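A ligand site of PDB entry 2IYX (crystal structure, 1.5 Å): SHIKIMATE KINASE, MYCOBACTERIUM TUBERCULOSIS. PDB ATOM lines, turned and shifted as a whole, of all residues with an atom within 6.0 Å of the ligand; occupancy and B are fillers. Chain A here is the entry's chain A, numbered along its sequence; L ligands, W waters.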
ATOM      1  N   PRO A  11     -22.581 -27.698 -20.497  1.00  0.00           N
ATOM      2  CA  PRO A  11     -23.245 -28.865 -20.006  1.00  0.00           C
ATOM      3  C   PRO A  11     -23.942 -29.607 -21.164  1.00  0.00           C
ATOM      4  O   PRO A  11     -24.516 -28.954 -22.032  1.00  0.00           O
ATOM      5  CB  PRO A  11     -24.321 -28.299 -19.048  1.00  0.00           C
ATOM      6  CG  PRO A  11     -23.973 -26.876 -18.841  1.00  0.00           C
ATOM      7  CD  PRO A  11     -23.024 -26.441 -19.857  1.00  0.00           C
ATOM      8  N   LYS A  15     -18.468 -33.876 -21.779  1.00  0.00           N
ATOM      9  CA  LYS A  15     -17.229 -33.862 -20.997  1.00  0.00           C
ATOM     10  C   LYS A  15     -17.012 -35.107 -20.137  1.00  0.00           C
ATOM     11  O   LYS A  15     -15.908 -35.638 -20.069  1.00  0.00           O
ATOM     12  CB  LYS A  15     -17.127 -32.577 -20.157  1.00  0.00           C
ATOM     13  CG  LYS A  15     -17.075 -31.269 -20.974  1.00  0.00           C
ATOM     14  CD  LYS A  15     -16.868 -30.052 -20.062  1.00  0.00           C
ATOM     15  CE  LYS A  15     -17.983 -29.829 -19.065  1.00  0.00           C
ATOM     16  NZ  LYS A  15     -19.310 -29.591 -19.721  1.00  0.00           N
ATOM     17  N   ASP A  34     -15.614 -29.922 -11.031  1.00  0.00           N
ATOM     18  CA  ASP A  34     -16.800 -29.815 -10.173  1.00  0.00           C
ATOM     19  C   ASP A  34     -16.635 -30.769  -9.002  1.00  0.00           C
ATOM     20  O   ASP A  34     -16.947 -30.408  -7.849  1.00  0.00           O
ATOM     21  CB  ASP A  34     -18.044 -30.181 -10.944  1.00  0.00           C
ATOM     22  CG  ASP A  34     -18.571 -29.070 -11.840  1.00  0.00           C
ATOM     23  OD1 ASP A  34     -18.139 -27.901 -11.742  1.00  0.00           O
ATOM     24  OD2 ASP A  34     -19.497 -29.413 -12.625  1.00  0.00           O
ATOM     25  N   ILE A  37     -14.145 -29.413  -6.563  1.00  0.00           N
ATOM     26  CA  ILE A  37     -14.714 -28.356  -5.719  1.00  0.00           C
ATOM     27  C   ILE A  37     -15.509 -28.984  -4.559  1.00  0.00           C
ATOM     28  O   ILE A  37     -15.414 -28.509  -3.432  1.00  0.00           O
ATOM     29  CB  ILE A  37     -15.610 -27.441  -6.557  1.00  0.00           C
ATOM     30  CG1 ILE A  37     -14.746 -26.571  -7.532  1.00  0.00           C
ATOM     31  CG2 ILE A  37     -16.512 -26.538  -5.708  1.00  0.00           C
ATOM     32  CD1 ILE A  37     -15.567 -25.891  -8.598  1.00  0.00           C
ATOM     33  N   ILE A  45     -22.302 -28.291  -5.027  1.00  0.00           N
ATOM     34  CA  ILE A  45     -22.276 -27.105  -5.902  1.00  0.00           C
ATOM     35  C   ILE A  45     -23.588 -26.304  -5.787  1.00  0.00           C
ATOM     36  O   ILE A  45     -23.596 -25.083  -5.650  1.00  0.00           O
ATOM     37  CB  ILE A  45     -21.955 -27.465  -7.303  1.00  0.00           C
ATOM     38  CG1 ILE A  45     -20.444 -27.857  -7.331  1.00  0.00           C
ATOM     39  CG2 ILE A  45     -22.213 -26.285  -8.262  1.00  0.00           C
ATOM     40  CD1 ILE A  45     -19.895 -28.162  -8.657  1.00  0.00           C
ATOM     41  N   PHE A  49     -24.025 -22.239  -4.730  1.00  0.00           N
ATOM     42  CA  PHE A  49     -24.789 -21.266  -5.514  1.00  0.00           C
ATOM     43  C   PHE A  49     -25.956 -20.656  -4.680  1.00  0.00           C
ATOM     44  O   PHE A  49     -26.149 -19.439  -4.682  1.00  0.00           O
ATOM     45  CB  PHE A  49     -25.369 -21.887  -6.766  1.00  0.00           C
ATOM     46  CG  PHE A  49     -24.468 -21.799  -7.983  1.00  0.00           C
ATOM     47  CD1 PHE A  49     -23.435 -22.713  -8.160  1.00  0.00           C
ATOM     48  CD2 PHE A  49     -24.672 -20.860  -8.985  1.00  0.00           C
ATOM     49  CE1 PHE A  49     -22.659 -22.690  -9.280  1.00  0.00           C
ATOM     50  CE2 PHE A  49     -23.848 -20.801 -10.109  1.00  0.00           C
ATOM     51  CZ  PHE A  49     -22.857 -21.723 -10.255  1.00  0.00           C
ATOM     52  N   GLU A  54     -23.239 -17.142  -7.048  1.00  0.00           N
ATOM     53  CA  GLU A  54     -22.393 -17.531  -8.157  1.00  0.00           C
ATOM     54  C   GLU A  54     -20.997 -16.900  -8.096  1.00  0.00           C
ATOM     55  O   GLU A  54     -19.981 -17.556  -8.457  1.00  0.00           O
ATOM     56  CB  GLU A  54     -23.037 -17.220  -9.499  1.00  0.00           C
ATOM     57  CG  GLU A  54     -22.180 -17.676 -10.689  1.00  0.00           C
ATOM     58  CD  GLU A  54     -22.861 -17.513 -12.017  1.00  0.00           C
ATOM     59  OE1 GLU A  54     -24.051 -17.130 -12.087  1.00  0.00           O
ATOM     60  OE2 GLU A  54     -22.156 -17.785 -13.024  1.00  0.00           O
ATOM     61  N   PHE A  57     -18.868 -18.909  -5.929  1.00  0.00           N
ATOM     62  CA  PHE A  57     -18.598 -20.164  -6.645  1.00  0.00           C
ATOM     63  C   PHE A  57     -17.424 -19.991  -7.667  1.00  0.00           C
ATOM     64  O   PHE A  57     -16.534 -20.845  -7.741  1.00  0.00           O
ATOM     65  CB  PHE A  57     -19.820 -20.693  -7.371  1.00  0.00           C
ATOM     66  CG  PHE A  57     -19.523 -21.934  -8.151  1.00  0.00           C
ATOM     67  CD1 PHE A  57     -19.364 -23.133  -7.496  1.00  0.00           C
ATOM     68  CD2 PHE A  57     -19.226 -21.893  -9.505  1.00  0.00           C
ATOM     69  CE1 PHE A  57     -19.029 -24.273  -8.169  1.00  0.00           C
ATOM     70  CE2 PHE A  57     -18.946 -23.055 -10.187  1.00  0.00           C
ATOM     71  CZ  PHE A  57     -18.857 -24.221  -9.534  1.00  0.00           C
ATOM     72  N   ARG A  58     -17.491 -18.936  -8.473  1.00  0.00           N
ATOM     73  CA  ARG A  58     -16.483 -18.734  -9.542  1.00  0.00           C
ATOM     74  C   ARG A  58     -15.089 -18.530  -8.976  1.00  0.00           C
ATOM     75  O   ARG A  58     -14.137 -18.989  -9.579  1.00  0.00           O
ATOM     76  CB  ARG A  58     -16.873 -17.576 -10.433  1.00  0.00           C
ATOM     77  CG  ARG A  58     -18.199 -17.817 -11.194  1.00  0.00           C
ATOM     78  CD  ARG A  58     -18.082 -18.914 -12.176  1.00  0.00           C
ATOM     79  NE  ARG A  58     -19.350 -19.188 -12.861  1.00  0.00           N
ATOM     80  CZ  ARG A  58     -19.738 -20.344 -13.358  1.00  0.00           C
ATOM     81  NH1 ARG A  58     -18.934 -21.384 -13.367  1.00  0.00           N
ATOM     82  NH2 ARG A  58     -20.984 -20.461 -13.847  1.00  0.00           N
ATOM     83  N   GLU A  61     -13.975 -21.966  -7.861  1.00  0.00           N
ATOM     84  CA  GLU A  61     -13.720 -22.748  -9.052  1.00  0.00           C
ATOM     85  C   GLU A  61     -12.382 -22.366  -9.690  1.00  0.00           C
ATOM     86  O   GLU A  61     -11.629 -23.232 -10.136  1.00  0.00           O
ATOM     87  CB  GLU A  61     -14.876 -22.476 -10.028  1.00  0.00           C
ATOM     88  CG  GLU A  61     -14.724 -23.207 -11.345  1.00  0.00           C
ATOM     89  CD  GLU A  61     -15.915 -22.934 -12.299  1.00  0.00           C
ATOM     90  OE1 GLU A  61     -16.265 -21.742 -12.512  1.00  0.00           O
ATOM     91  OE2 GLU A  61     -16.412 -23.978 -12.782  1.00  0.00           O
ATOM     92  N   LEU A  78     -13.350 -29.250 -17.181  1.00  0.00           N
ATOM     93  CA  LEU A  78     -13.729 -28.076 -16.444  1.00  0.00           C
ATOM     94  C   LEU A  78     -15.224 -27.910 -16.438  1.00  0.00           C
ATOM     95  O   LEU A  78     -15.883 -28.059 -17.483  1.00  0.00           O
ATOM     96  CB  LEU A  78     -13.140 -26.784 -17.043  1.00  0.00           C
ATOM     97  CG  LEU A  78     -11.645 -26.688 -17.271  1.00  0.00           C
ATOM     98  CD1 LEU A  78     -11.228 -25.186 -17.565  1.00  0.00           C
ATOM     99  CD2 LEU A  78     -10.824 -27.265 -16.137  1.00  0.00           C
ATOM    100  N   GLY A  79     -15.773 -27.436 -15.341  1.00  0.00           N
ATOM    101  CA  GLY A  79     -17.183 -27.116 -15.308  1.00  0.00           C
ATOM    102  C   GLY A  79     -17.534 -26.127 -16.411  1.00  0.00           C
ATOM    103  O   GLY A  79     -16.720 -25.309 -16.802  1.00  0.00           O
ATOM    104  N   GLY A  80     -18.766 -26.171 -16.891  1.00  0.00           N
ATOM    105  CA  GLY A  80     -19.158 -25.446 -18.092  1.00  0.00           C
ATOM    106  C   GLY A  80     -18.940 -23.980 -18.084  1.00  0.00           C
ATOM    107  O   GLY A  80     -18.748 -23.349 -19.116  1.00  0.00           O
ATOM    108  N   GLY A  81     -19.014 -23.373 -16.920  1.00  0.00           N
ATOM    109  CA  GLY A  81     -18.864 -21.937 -16.793  1.00  0.00           C
ATOM    110  C   GLY A  81     -17.488 -21.441 -16.373  1.00  0.00           C
ATOM    111  O   GLY A  81     -17.276 -20.257 -16.194  1.00  0.00           O
ATOM    112  N   ALA A  82     -16.521 -22.356 -16.173  1.00  0.00           N
ATOM    113  CA  ALA A  82     -15.230 -21.917 -15.718  1.00  0.00           C
ATOM    114  C   ALA A  82     -14.581 -20.884 -16.675  1.00  0.00           C
ATOM    115  O   ALA A  82     -13.896 -19.957 -16.206  1.00  0.00           O
ATOM    116  CB  ALA A  82     -14.348 -23.114 -15.514  1.00  0.00           C
ATOM    117  N   VAL A 116     -29.260 -31.737 -10.778  1.00  0.00           N
ATOM    118  CA  VAL A 116     -29.443 -30.378 -10.319  1.00  0.00           C
ATOM    119  C   VAL A 116     -28.446 -29.494 -11.066  1.00  0.00           C
ATOM    120  O   VAL A 116     -27.235 -29.771 -11.064  1.00  0.00           O
ATOM    121  CB  VAL A 116     -29.200 -30.253  -8.801  1.00  0.00           C
ATOM    122  CG1 VAL A 116     -29.345 -28.861  -8.342  1.00  0.00           C
ATOM    123  CG2 VAL A 116     -30.207 -31.147  -8.028  1.00  0.00           C
ATOM    124  N   ARG A 117     -28.968 -28.439 -11.704  1.00  0.00           N
ATOM    125  CA  ARG A 117     -28.172 -27.494 -12.492  1.00  0.00           C
ATOM    126  C   ARG A 117     -28.623 -26.073 -12.161  1.00  0.00           C
ATOM    127  O   ARG A 117     -29.609 -25.570 -12.734  1.00  0.00           O
ATOM    128  CB  ARG A 117     -28.404 -27.800 -13.945  1.00  0.00           C
ATOM    129  CG  ARG A 117     -28.104 -29.180 -14.367  1.00  0.00           C
ATOM    130  CD  ARG A 117     -28.285 -29.339 -15.880  1.00  0.00           C
ATOM    131  NE  ARG A 117     -28.301 -30.740 -16.335  1.00  0.00           N
ATOM    132  CZ  ARG A 117     -27.201 -31.402 -16.624  1.00  0.00           C
ATOM    133  NH1 ARG A 117     -26.048 -30.800 -16.502  1.00  0.00           N
ATOM    134  NH2 ARG A 117     -27.262 -32.669 -17.030  1.00  0.00           N
ATOM    135  N   PRO A 118     -27.949 -25.394 -11.222  1.00  0.00           N
ATOM    136  CA  PRO A 118     -28.364 -24.025 -10.875  1.00  0.00           C
ATOM    137  C   PRO A 118     -28.627 -23.086 -12.022  1.00  0.00           C
ATOM    138  O   PRO A 118     -29.546 -22.236 -11.967  1.00  0.00           O
ATOM    139  CB  PRO A 118     -27.254 -23.564  -9.967  1.00  0.00           C
ATOM    140  CG  PRO A 118     -26.682 -24.853  -9.378  1.00  0.00           C
ATOM    141  CD  PRO A 118     -26.825 -25.883 -10.408  1.00  0.00           C
ATOM    142  N   LEU A 119     -27.828 -23.206 -13.090  1.00  0.00           N
ATOM    143  CA  LEU A 119     -27.920 -22.237 -14.207  1.00  0.00           C
ATOM    144  C   LEU A 119     -28.691 -22.861 -15.366  1.00  0.00           C
ATOM    145  O   LEU A 119     -28.788 -22.231 -16.441  1.00  0.00           O
ATOM    146  CB  LEU A 119     -26.519 -21.780 -14.634  1.00  0.00           C
ATOM    147  CG  LEU A 119     -25.766 -21.033 -13.552  1.00  0.00           C
ATOM    148  CD1 LEU A 119     -24.427 -20.577 -14.108  1.00  0.00           C
ATOM    149  CD2 LEU A 119     -26.533 -19.940 -12.972  1.00  0.00           C
ATOM    150  N   LEU A 120     -29.293 -24.038 -15.212  1.00  0.00           N
ATOM    151  CA  LEU A 120     -30.060 -24.645 -16.274  1.00  0.00           C
ATOM    152  C   LEU A 120     -31.246 -25.418 -15.681  1.00  0.00           C
ATOM    153  O   LEU A 120     -31.311 -26.660 -15.735  1.00  0.00           O
ATOM    154  CB  LEU A 120     -29.221 -25.640 -17.044  1.00  0.00           C
ATOM    155  CG  LEU A 120     -28.189 -25.118 -18.009  1.00  0.00           C
ATOM    156  CD1 LEU A 120     -27.502 -26.304 -18.664  1.00  0.00           C
ATOM    157  CD2 LEU A 120     -28.885 -24.223 -19.035  1.00  0.00           C
ATOM    158  N   LEU A 132     -26.600 -19.244 -22.520  1.00  0.00           N
ATOM    159  CA  LEU A 132     -25.238 -19.716 -22.084  1.00  0.00           C
ATOM    160  C   LEU A 132     -24.384 -19.948 -23.327  1.00  0.00           C
ATOM    161  O   LEU A 132     -23.226 -19.536 -23.375  1.00  0.00           O
ATOM    162  CB  LEU A 132     -25.325 -20.986 -21.284  1.00  0.00           C
ATOM    163  CG  LEU A 132     -26.038 -20.904 -19.937  1.00  0.00           C
ATOM    164  CD1 LEU A 132     -25.936 -22.280 -19.335  1.00  0.00           C
ATOM    165  CD2 LEU A 132     -25.455 -19.872 -19.031  1.00  0.00           C
ATOM    166  N   ARG A 136     -21.000 -17.897 -24.130  1.00  0.00           N
ATOM    167  CA  ARG A 136     -19.768 -18.650 -23.854  1.00  0.00           C
ATOM    168  C   ARG A 136     -19.001 -19.087 -25.099  1.00  0.00           C
ATOM    169  O   ARG A 136     -17.778 -19.346 -25.004  1.00  0.00           O
ATOM    170  CB  ARG A 136     -20.039 -19.835 -22.965  1.00  0.00           C
ATOM    171  CG  ARG A 136     -20.540 -19.413 -21.582  1.00  0.00           C
ATOM    172  CD  ARG A 136     -20.940 -20.591 -20.740  1.00  0.00           C
ATOM    173  NE  ARG A 136     -21.443 -20.180 -19.418  1.00  0.00           N
ATOM    174  CZ  ARG A 136     -21.862 -21.064 -18.508  1.00  0.00           C
ATOM    175  NH1 ARG A 136     -21.816 -22.347 -18.737  1.00  0.00           N
ATOM    176  NH2 ARG A 136     -22.302 -20.606 -17.364  1.00  0.00           N
ATOM    177  N   TYR A 140     -14.981 -20.250 -25.099  1.00  0.00           N
ATOM    178  CA  TYR A 140     -14.503 -21.554 -25.425  1.00  0.00           C
ATOM    179  C   TYR A 140     -13.514 -21.520 -26.609  1.00  0.00           C
ATOM    180  O   TYR A 140     -12.413 -22.116 -26.547  1.00  0.00           O
ATOM    181  CB  TYR A 140     -15.651 -22.537 -25.769  1.00  0.00           C
ATOM    182  CG  TYR A 140     -16.602 -22.862 -24.661  1.00  0.00           C
ATOM    183  CD1 TYR A 140     -16.164 -23.325 -23.403  1.00  0.00           C
ATOM    184  CD2 TYR A 140     -17.966 -22.738 -24.859  1.00  0.00           C
ATOM    185  CE1 TYR A 140     -17.095 -23.635 -22.402  1.00  0.00           C
ATOM    186  CE2 TYR A 140     -18.872 -23.038 -23.846  1.00  0.00           C
ATOM    187  CZ  TYR A 140     -18.426 -23.469 -22.637  1.00  0.00           C
ATOM    188  OH  TYR A 140     -19.377 -23.751 -21.674  1.00  0.00           O
HETATM  189  O1  LIG L   1     -19.870 -26.078 -12.590  1.00  0.00           O
HETATM  190  C1  LIG L   1     -21.238 -26.510 -12.557  1.00  0.00           C
HETATM  191  C2  LIG L   1     -22.097 -25.321 -12.138  1.00  0.00           C
HETATM  192  O2  LIG L   1     -23.464 -25.738 -11.990  1.00  0.00           O
HETATM  193  C3  LIG L   1     -22.031 -24.200 -13.157  1.00  0.00           C
HETATM  194  C4  LIG L   1     -22.121 -24.711 -14.553  1.00  0.00           C
HETATM  195  C5  LIG L   1     -22.257 -23.709 -15.606  1.00  0.00           C
HETATM  196  O3  LIG L   1     -22.659 -24.110 -16.762  1.00  0.00           O
HETATM  197  O4  LIG L   1     -21.877 -22.540 -15.366  1.00  0.00           O
HETATM  198  C6  LIG L   1     -21.945 -25.990 -14.918  1.00  0.00           C
HETATM  199  C7  LIG L   1     -21.674 -27.063 -13.912  1.00  0.00           C
HETATM  200  O5  LIG L   1     -20.679 -28.008 -14.409  1.00  0.00           O
HETATM  201  O   HOH W   1     -20.555 -28.750 -17.369  1.00  0.00           O
HETATM  202  O   HOH W   2     -18.731 -24.158 -14.173  1.00  0.00           O
HETATM  203  O   HOH W   3     -23.712 -28.325 -10.756  1.00  0.00           O
HETATM  204  O   HOH W   4     -25.220 -25.372 -16.178  1.00  0.00           O
HETATM  205  O   HOH W   5     -25.770 -25.056 -13.579  1.00  0.00           O
HETATM  206  O   HOH W   6     -22.646 -29.293 -16.038  1.00  0.00           O
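O5 of the ligand is in hydrogen-bond range of OD2 of Asp 34 (2.6 Å). The guanidinium group (NH2) of Arg 58 is in salt-bridge range of an oxygen (O4) of the ligand, at 2.7 Å. The guanidinium group of Arg 136 is in salt-bridge range of an oxygen (O3) of the ligand. O4 of the ligand is in hydrogen-bond range of N of Gly 81 (3.4 Å).
The guanidinium group of Arg 58 lies close to the backbone carbonyl oxygen of Gly 81 (3.5 Å). The guanidinium group of Arg 58 lies within salt-bridge range of the side-chain carboxylate of Glu 61, at 2.8 Å. The guanidinium group (NH2) of Arg 58 lies within salt-bridge range of the side-chain carboxylate (OE2) of Glu 54, at 3.0 Å. The backbone carbonyl oxygen (O) of Gly 80 is in hydrogen-bond range of the guanidinium group (NH1) of Arg 136, 3.2 Å away. The side-chain hydroxyl of Tyr 140 is in hydrogen-bond range of the backbone carbonyl oxygen of Gly 80, at 2.7 Å.
CG of Pro 11 touches O3 of the ligand, at 3.7 Å. Ile 45 touches the ligand (CG2 to O2, 3.97 Å). CZ of Phe 49 touches C3 of the ligand, 3.9 Å away. Phe 57 touches the ligand. Gly 79 touches the ligand (CA to O5, 3.7 Å). Gly 80 touches the ligand. Pro 118 touches the ligand (CD to O2, 3.7 Å). CD1 of Leu 119 touches O4 of the ligand (3.5 Å). Hydrophobic or aromatic side chains that line the ligand: Pro 11, Ile 45, Phe 49, Phe 57, Pro 118 and Leu 119. The nearest printed residue that does not touch the ligand is Glu 61 (4.1 Å).
Water W5 lies within hydrogen-bond range of N of Leu 119 and O2 of the ligand. Water W1 lies within hydrogen-bond range of NZ of Lys 15 (2.8 Å), O5 of the ligand (3.1 Å) and N of Gly 80 (3.2 Å).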
